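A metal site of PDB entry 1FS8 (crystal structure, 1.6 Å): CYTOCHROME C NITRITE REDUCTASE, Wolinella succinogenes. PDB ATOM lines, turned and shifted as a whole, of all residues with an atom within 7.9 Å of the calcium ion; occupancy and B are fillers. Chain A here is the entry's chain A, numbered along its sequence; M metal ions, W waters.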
ATOM      1  N   TYR A  68     -27.096 -42.212 -21.312  1.00  0.00           N
ATOM      2  CA  TYR A  68     -26.051 -41.205 -21.227  1.00  0.00           C
ATOM      3  C   TYR A  68     -25.300 -41.373 -19.898  1.00  0.00           C
ATOM      4  O   TYR A  68     -25.863 -41.862 -18.927  1.00  0.00           O
ATOM      5  CB  TYR A  68     -26.707 -39.817 -21.325  1.00  0.00           C
ATOM      6  CG  TYR A  68     -25.799 -38.690 -21.748  1.00  0.00           C
ATOM      7  CD1 TYR A  68     -25.077 -38.745 -22.929  1.00  0.00           C
ATOM      8  CD2 TYR A  68     -25.700 -37.530 -20.971  1.00  0.00           C
ATOM      9  CE1 TYR A  68     -24.266 -37.687 -23.335  1.00  0.00           C
ATOM     10  CE2 TYR A  68     -24.906 -36.468 -21.364  1.00  0.00           C
ATOM     11  CZ  TYR A  68     -24.194 -36.544 -22.545  1.00  0.00           C
ATOM     12  OH  TYR A  68     -23.400 -35.491 -22.920  1.00  0.00           O
ATOM     13  N   VAL A 194     -20.484 -22.291 -17.979  1.00  0.00           N
ATOM     14  CA  VAL A 194     -21.316 -22.059 -19.150  1.00  0.00           C
ATOM     15  C   VAL A 194     -21.713 -23.394 -19.781  1.00  0.00           C
ATOM     16  O   VAL A 194     -21.127 -24.436 -19.463  1.00  0.00           O
ATOM     17  CB  VAL A 194     -20.555 -21.243 -20.223  1.00  0.00           C
ATOM     18  CG1 VAL A 194     -20.359 -19.801 -19.757  1.00  0.00           C
ATOM     19  CG2 VAL A 194     -19.203 -21.902 -20.508  1.00  0.00           C
ATOM     20  N   GLU A 195     -22.697 -23.360 -20.665  1.00  0.00           N
ATOM     21  CA  GLU A 195     -23.148 -24.557 -21.370  1.00  0.00           C
ATOM     22  C   GLU A 195     -22.267 -24.732 -22.600  1.00  0.00           C
ATOM     23  O   GLU A 195     -21.809 -23.756 -23.197  1.00  0.00           O
ATOM     24  CB  GLU A 195     -24.629 -24.425 -21.761  1.00  0.00           C
ATOM     25  CG  GLU A 195     -25.045 -24.996 -23.116  1.00  0.00           C
ATOM     26  CD  GLU A 195     -24.967 -26.515 -23.207  1.00  0.00           C
ATOM     27  OE1 GLU A 195     -24.775 -27.199 -22.184  1.00  0.00           O
ATOM     28  OE2 GLU A 195     -25.103 -27.033 -24.332  1.00  0.00           O
ATOM     29  N   TYR A 196     -21.995 -25.978 -22.947  1.00  0.00           N
ATOM     30  CA  TYR A 196     -21.123 -26.266 -24.079  1.00  0.00           C
ATOM     31  C   TYR A 196     -21.489 -27.606 -24.711  1.00  0.00           C
ATOM     32  O   TYR A 196     -22.351 -28.329 -24.228  1.00  0.00           O
ATOM     33  CB  TYR A 196     -19.674 -26.363 -23.602  1.00  0.00           C
ATOM     34  CG  TYR A 196     -19.449 -27.622 -22.786  1.00  0.00           C
ATOM     35  CD1 TYR A 196     -19.810 -27.694 -21.437  1.00  0.00           C
ATOM     36  CD2 TYR A 196     -18.983 -28.787 -23.392  1.00  0.00           C
ATOM     37  CE1 TYR A 196     -19.726 -28.893 -20.718  1.00  0.00           C
ATOM     38  CE2 TYR A 196     -18.904 -29.989 -22.686  1.00  0.00           C
ATOM     39  CZ  TYR A 196     -19.268 -30.035 -21.357  1.00  0.00           C
ATOM     40  OH  TYR A 196     -19.205 -31.234 -20.684  1.00  0.00           O
ATOM     41  N   TYR A 197     -20.801 -27.897 -25.804  1.00  0.00           N
ATOM     42  CA  TYR A 197     -20.945 -29.173 -26.486  1.00  0.00           C
ATOM     43  C   TYR A 197     -19.579 -29.442 -27.117  1.00  0.00           C
ATOM     44  O   TYR A 197     -18.758 -28.533 -27.217  1.00  0.00           O
ATOM     45  CB  TYR A 197     -22.053 -29.142 -27.558  1.00  0.00           C
ATOM     46  CG  TYR A 197     -21.730 -28.449 -28.869  1.00  0.00           C
ATOM     47  CD1 TYR A 197     -21.871 -27.076 -29.006  1.00  0.00           C
ATOM     48  CD2 TYR A 197     -21.349 -29.190 -29.986  1.00  0.00           C
ATOM     49  CE1 TYR A 197     -21.654 -26.451 -30.243  1.00  0.00           C
ATOM     50  CE2 TYR A 197     -21.128 -28.587 -31.212  1.00  0.00           C
ATOM     51  CZ  TYR A 197     -21.279 -27.214 -31.338  1.00  0.00           C
ATOM     52  OH  TYR A 197     -21.071 -26.614 -32.566  1.00  0.00           O
ATOM     53  N   PHE A 198     -19.337 -30.688 -27.499  1.00  0.00           N
ATOM     54  CA  PHE A 198     -18.072 -31.053 -28.127  1.00  0.00           C
ATOM     55  C   PHE A 198     -18.257 -31.087 -29.629  1.00  0.00           C
ATOM     56  O   PHE A 198     -19.128 -31.785 -30.132  1.00  0.00           O
ATOM     57  CB  PHE A 198     -17.599 -32.426 -27.673  1.00  0.00           C
ATOM     58  CG  PHE A 198     -17.255 -32.516 -26.211  1.00  0.00           C
ATOM     59  CD1 PHE A 198     -16.606 -31.472 -25.561  1.00  0.00           C
ATOM     60  CD2 PHE A 198     -17.564 -33.665 -25.488  1.00  0.00           C
ATOM     61  CE1 PHE A 198     -16.261 -31.573 -24.219  1.00  0.00           C
ATOM     62  CE2 PHE A 198     -17.223 -33.779 -24.141  1.00  0.00           C
ATOM     63  CZ  PHE A 198     -16.574 -32.730 -23.499  1.00  0.00           C
ATOM     64  N   THR A 217     -17.152 -26.189 -27.326  1.00  0.00           N
ATOM     65  CA  THR A 217     -17.758 -25.132 -28.114  1.00  0.00           C
ATOM     66  C   THR A 217     -18.993 -24.588 -27.422  1.00  0.00           C
ATOM     67  O   THR A 217     -19.855 -25.357 -26.998  1.00  0.00           O
ATOM     68  CB  THR A 217     -18.155 -25.673 -29.497  1.00  0.00           C
ATOM     69  OG1 THR A 217     -17.027 -26.319 -30.099  1.00  0.00           O
ATOM     70  CG2 THR A 217     -18.632 -24.549 -30.404  1.00  0.00           C
ATOM     71  N   PRO A 219     -22.470 -23.008 -27.632  1.00  0.00           N
ATOM     72  CA  PRO A 219     -23.563 -22.899 -28.605  1.00  0.00           C
ATOM     73  C   PRO A 219     -24.225 -21.523 -28.607  1.00  0.00           C
ATOM     74  O   PRO A 219     -25.449 -21.424 -28.542  1.00  0.00           O
ATOM     75  CB  PRO A 219     -24.524 -23.987 -28.150  1.00  0.00           C
ATOM     76  CG  PRO A 219     -24.416 -23.877 -26.655  1.00  0.00           C
ATOM     77  CD  PRO A 219     -22.909 -23.771 -26.442  1.00  0.00           C
ATOM     78  N   MET A 229     -30.216 -21.186 -28.275  1.00  0.00           N
ATOM     79  CA  MET A 229     -29.288 -22.322 -28.294  1.00  0.00           C
ATOM     80  C   MET A 229     -30.009 -23.534 -28.867  1.00  0.00           C
ATOM     81  O   MET A 229     -29.413 -24.371 -29.530  1.00  0.00           O
ATOM     82  CB  MET A 229     -28.807 -22.669 -26.887  1.00  0.00           C
ATOM     83  CG  MET A 229     -27.997 -21.611 -26.202  1.00  0.00           C
ATOM     84  SD  MET A 229     -27.347 -22.288 -24.662  1.00  0.00           S
ATOM     85  CE  MET A 229     -26.221 -21.043 -24.208  1.00  0.00           C
ATOM     86  N   TYR A 233     -28.723 -25.844 -32.001  1.00  0.00           N
ATOM     87  CA  TYR A 233     -28.568 -27.295 -32.041  1.00  0.00           C
ATOM     88  C   TYR A 233     -29.448 -27.968 -33.089  1.00  0.00           C
ATOM     89  O   TYR A 233     -29.016 -28.930 -33.722  1.00  0.00           O
ATOM     90  CB  TYR A 233     -28.862 -27.892 -30.655  1.00  0.00           C
ATOM     91  CG  TYR A 233     -27.752 -27.668 -29.650  1.00  0.00           C
ATOM     92  CD1 TYR A 233     -26.449 -28.102 -29.916  1.00  0.00           C
ATOM     93  CD2 TYR A 233     -28.003 -27.037 -28.429  1.00  0.00           C
ATOM     94  CE1 TYR A 233     -25.424 -27.932 -28.977  1.00  0.00           C
ATOM     95  CE2 TYR A 233     -26.988 -26.863 -27.488  1.00  0.00           C
ATOM     96  CZ  TYR A 233     -25.707 -27.316 -27.765  1.00  0.00           C
ATOM     97  OH  TYR A 233     -24.700 -27.153 -26.842  1.00  0.00           O
ATOM     98  N   PHE A 238     -27.868 -31.546 -34.284  1.00  0.00           N
ATOM     99  CA  PHE A 238     -26.993 -32.100 -33.252  1.00  0.00           C
ATOM    100  C   PHE A 238     -27.753 -32.867 -32.175  1.00  0.00           C
ATOM    101  O   PHE A 238     -28.904 -32.563 -31.861  1.00  0.00           O
ATOM    102  CB  PHE A 238     -26.204 -30.978 -32.589  1.00  0.00           C
ATOM    103  CG  PHE A 238     -25.157 -31.475 -31.612  1.00  0.00           C
ATOM    104  CD1 PHE A 238     -23.936 -31.945 -32.071  1.00  0.00           C
ATOM    105  CD2 PHE A 238     -25.408 -31.465 -30.249  1.00  0.00           C
ATOM    106  CE1 PHE A 238     -22.972 -32.414 -31.171  1.00  0.00           C
ATOM    107  CE2 PHE A 238     -24.457 -31.917 -29.341  1.00  0.00           C
ATOM    108  CZ  PHE A 238     -23.228 -32.387 -29.811  1.00  0.00           C
ATOM    109  N   ASP A 240     -26.613 -34.989 -28.355  1.00  0.00           N
ATOM    110  CA  ASP A 240     -25.568 -35.431 -27.451  1.00  0.00           C
ATOM    111  C   ASP A 240     -25.618 -36.943 -27.325  1.00  0.00           C
ATOM    112  O   ASP A 240     -24.586 -37.597 -27.138  1.00  0.00           O
ATOM    113  CB  ASP A 240     -25.713 -34.760 -26.092  1.00  0.00           C
ATOM    114  CG  ASP A 240     -25.219 -33.327 -26.088  1.00  0.00           C
ATOM    115  OD1 ASP A 240     -23.995 -33.131 -26.220  1.00  0.00           O
ATOM    116  OD2 ASP A 240     -26.047 -32.401 -25.986  1.00  0.00           O
ATOM    117  N   LEU A 251     -30.489 -33.514 -26.166  1.00  0.00           N
ATOM    118  CA  LEU A 251     -29.529 -32.436 -25.955  1.00  0.00           C
ATOM    119  C   LEU A 251     -29.293 -32.366 -24.455  1.00  0.00           C
ATOM    120  O   LEU A 251     -30.245 -32.418 -23.668  1.00  0.00           O
ATOM    121  CB  LEU A 251     -30.087 -31.092 -26.427  1.00  0.00           C
ATOM    122  CG  LEU A 251     -30.240 -30.885 -27.933  1.00  0.00           C
ATOM    123  CD1 LEU A 251     -30.922 -29.555 -28.178  1.00  0.00           C
ATOM    124  CD2 LEU A 251     -28.871 -30.918 -28.595  1.00  0.00           C
ATOM    125  N   LYS A 252     -28.026 -32.284 -24.057  1.00  0.00           N
ATOM    126  CA  LYS A 252     -27.677 -32.195 -22.646  1.00  0.00           C
ATOM    127  C   LYS A 252     -27.269 -30.783 -22.281  1.00  0.00           C
ATOM    128  O   LYS A 252     -26.360 -30.206 -22.898  1.00  0.00           O
ATOM    129  CB  LYS A 252     -26.520 -33.138 -22.304  1.00  0.00           C
ATOM    130  CG  LYS A 252     -26.166 -33.149 -20.811  1.00  0.00           C
ATOM    131  CD  LYS A 252     -27.186 -33.939 -19.993  1.00  0.00           C
ATOM    132  CE  LYS A 252     -26.988 -33.758 -18.491  1.00  0.00           C
ATOM    133  NZ  LYS A 252     -27.443 -32.415 -18.006  1.00  0.00           N
ATOM    134  N   ALA A 253     -27.922 -30.208 -21.272  1.00  0.00           N
ATOM    135  CA  ALA A 253     -27.567 -28.874 -20.826  1.00  0.00           C
ATOM    136  C   ALA A 253     -26.586 -29.067 -19.674  1.00  0.00           C
ATOM    137  O   ALA A 253     -26.777 -29.949 -18.837  1.00  0.00           O
ATOM    138  CB  ALA A 253     -28.803 -28.134 -20.347  1.00  0.00           C
ATOM    139  N   GLN A 254     -25.537 -28.264 -19.643  1.00  0.00           N
ATOM    140  CA  GLN A 254     -24.574 -28.350 -18.548  1.00  0.00           C
ATOM    141  C   GLN A 254     -24.287 -26.979 -17.981  1.00  0.00           C
ATOM    142  O   GLN A 254     -23.909 -26.061 -18.714  1.00  0.00           O
ATOM    143  CB  GLN A 254     -23.270 -29.004 -19.001  1.00  0.00           C
ATOM    144  CG  GLN A 254     -23.397 -30.482 -19.338  1.00  0.00           C
ATOM    145  CD  GLN A 254     -23.280 -30.746 -20.819  1.00  0.00           C
ATOM    146  OE1 GLN A 254     -23.659 -29.909 -21.639  1.00  0.00           O
ATOM    147  NE2 GLN A 254     -22.782 -31.911 -21.184  1.00  0.00           N
ATOM    148  N   HIS A 255     -24.508 -26.846 -16.688  1.00  0.00           N
ATOM    149  CA  HIS A 255     -24.258 -25.619 -15.938  1.00  0.00           C
ATOM    150  C   HIS A 255     -24.182 -24.328 -16.739  1.00  0.00           C
ATOM    151  O   HIS A 255     -23.105 -23.737 -16.890  1.00  0.00           O
ATOM    152  CB  HIS A 255     -22.950 -25.805 -15.149  1.00  0.00           C
ATOM    153  CG  HIS A 255     -21.883 -26.498 -15.926  1.00  0.00           C
ATOM    154  ND1 HIS A 255     -21.276 -25.927 -17.021  1.00  0.00           N
ATOM    155  CD2 HIS A 255     -21.353 -27.732 -15.805  1.00  0.00           C
ATOM    156  CE1 HIS A 255     -20.427 -26.792 -17.556  1.00  0.00           C
ATOM    157  NE2 HIS A 255     -20.457 -27.898 -16.836  1.00  0.00           N
ATOM    158  N   TRP A 369     -34.612 -30.228 -23.096  1.00  0.00           N
ATOM    159  CA  TRP A 369     -33.560 -29.240 -23.283  1.00  0.00           C
ATOM    160  C   TRP A 369     -33.889 -28.018 -22.439  1.00  0.00           C
ATOM    161  O   TRP A 369     -33.026 -27.478 -21.736  1.00  0.00           O
ATOM    162  CB  TRP A 369     -33.448 -28.821 -24.759  1.00  0.00           C
ATOM    163  CG  TRP A 369     -32.586 -27.601 -24.928  1.00  0.00           C
ATOM    164  CD1 TRP A 369     -32.995 -26.356 -25.336  1.00  0.00           C
ATOM    165  CD2 TRP A 369     -31.182 -27.480 -24.653  1.00  0.00           C
ATOM    166  NE1 TRP A 369     -31.939 -25.482 -25.323  1.00  0.00           N
ATOM    167  CE2 TRP A 369     -30.812 -26.139 -24.907  1.00  0.00           C
ATOM    168  CE3 TRP A 369     -30.209 -28.386 -24.206  1.00  0.00           C
ATOM    169  CZ2 TRP A 369     -29.501 -25.685 -24.739  1.00  0.00           C
ATOM    170  CZ3 TRP A 369     -28.902 -27.920 -24.031  1.00  0.00           C
ATOM    171  CH2 TRP A 369     -28.564 -26.589 -24.303  1.00  0.00           C
ATOM    172  N   ASP A 372     -33.788 -28.963 -18.580  1.00  0.00           N
ATOM    173  CA  ASP A 372     -32.418 -29.205 -18.150  1.00  0.00           C
ATOM    174  C   ASP A 372     -31.668 -27.857 -18.083  1.00  0.00           C
ATOM    175  O   ASP A 372     -30.906 -27.619 -17.148  1.00  0.00           O
ATOM    176  CB  ASP A 372     -31.736 -30.174 -19.109  1.00  0.00           C
ATOM    177  CG  ASP A 372     -30.575 -30.939 -18.467  1.00  0.00           C
ATOM    178  OD1 ASP A 372     -30.352 -30.807 -17.252  1.00  0.00           O
ATOM    179  OD2 ASP A 372     -29.895 -31.688 -19.193  1.00  0.00           O
ATOM    180  N   MET A 373     -31.901 -26.991 -19.065  1.00  0.00           N
ATOM    181  CA  MET A 373     -31.249 -25.681 -19.055  1.00  0.00           C
ATOM    182  C   MET A 373     -31.676 -24.904 -17.817  1.00  0.00           C
ATOM    183  O   MET A 373     -30.912 -24.116 -17.268  1.00  0.00           O
ATOM    184  CB  MET A 373     -31.605 -24.873 -20.311  1.00  0.00           C
ATOM    185  CG  MET A 373     -30.691 -25.118 -21.498  1.00  0.00           C
ATOM    186  SD  MET A 373     -28.993 -24.537 -21.228  1.00  0.00           S
ATOM    187  CE  MET A 373     -29.224 -22.785 -21.300  1.00  0.00           C
HETATM  188 CA    CA M   1     -24.411 -29.282 -23.629  1.00  0.00          CA
HETATM  189  O   HOH W   1     -25.401 -29.803 -25.781  1.00  0.00           O
HETATM  190  O   HOH W   2     -23.389 -31.266 -24.264  1.00  0.00           O
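Merely in contact with the calcium ion: Tyr 233 (3.9 Å).
The backbone NH (N) of Lys 252 lies within hydrogen-bond range of the side-chain carboxylate (OD2) of Asp 240 (2.8 Å).
O of Tyr 233 sits at hydrogen-bond distance from N of Phe 238 (2.9 Å).
The side-chain carboxylate (OD2) of Asp 372 lies within salt-bridge range of the side-chain amino group (NZ) of Lys 252 (2.8 Å).
The side-chain carboxylate (OE2) of Glu 195 lies close to the side-chain hydroxyl (OH) of Tyr 233.
Water W1 lies within hydrogen-bond range of the side-chain carboxylate (OD2) of Asp 240 (2.7 Å) and the side-chain hydroxyl (OH) of Tyr 233 (2.9 Å).
Water W2 bridges OD1 of Asp 240 and NE2 of Gln 254.
The calcium ion is bound by the side-chain amide oxygen (OE1) of Gln 254 (2.2 Å), the backbone carbonyl oxygen (O) of Lys 252 (2.3 Å), water W2 (2.3 Å), the backbone carbonyl oxygen (O) of Tyr 196 (2.3 Å), water W1 (2.4 Å), the side-chain carboxylate (OE2) of Glu 195 (2.5 Å) and the side-chain carboxylate (OE1) of Glu 195 (2.6 Å).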
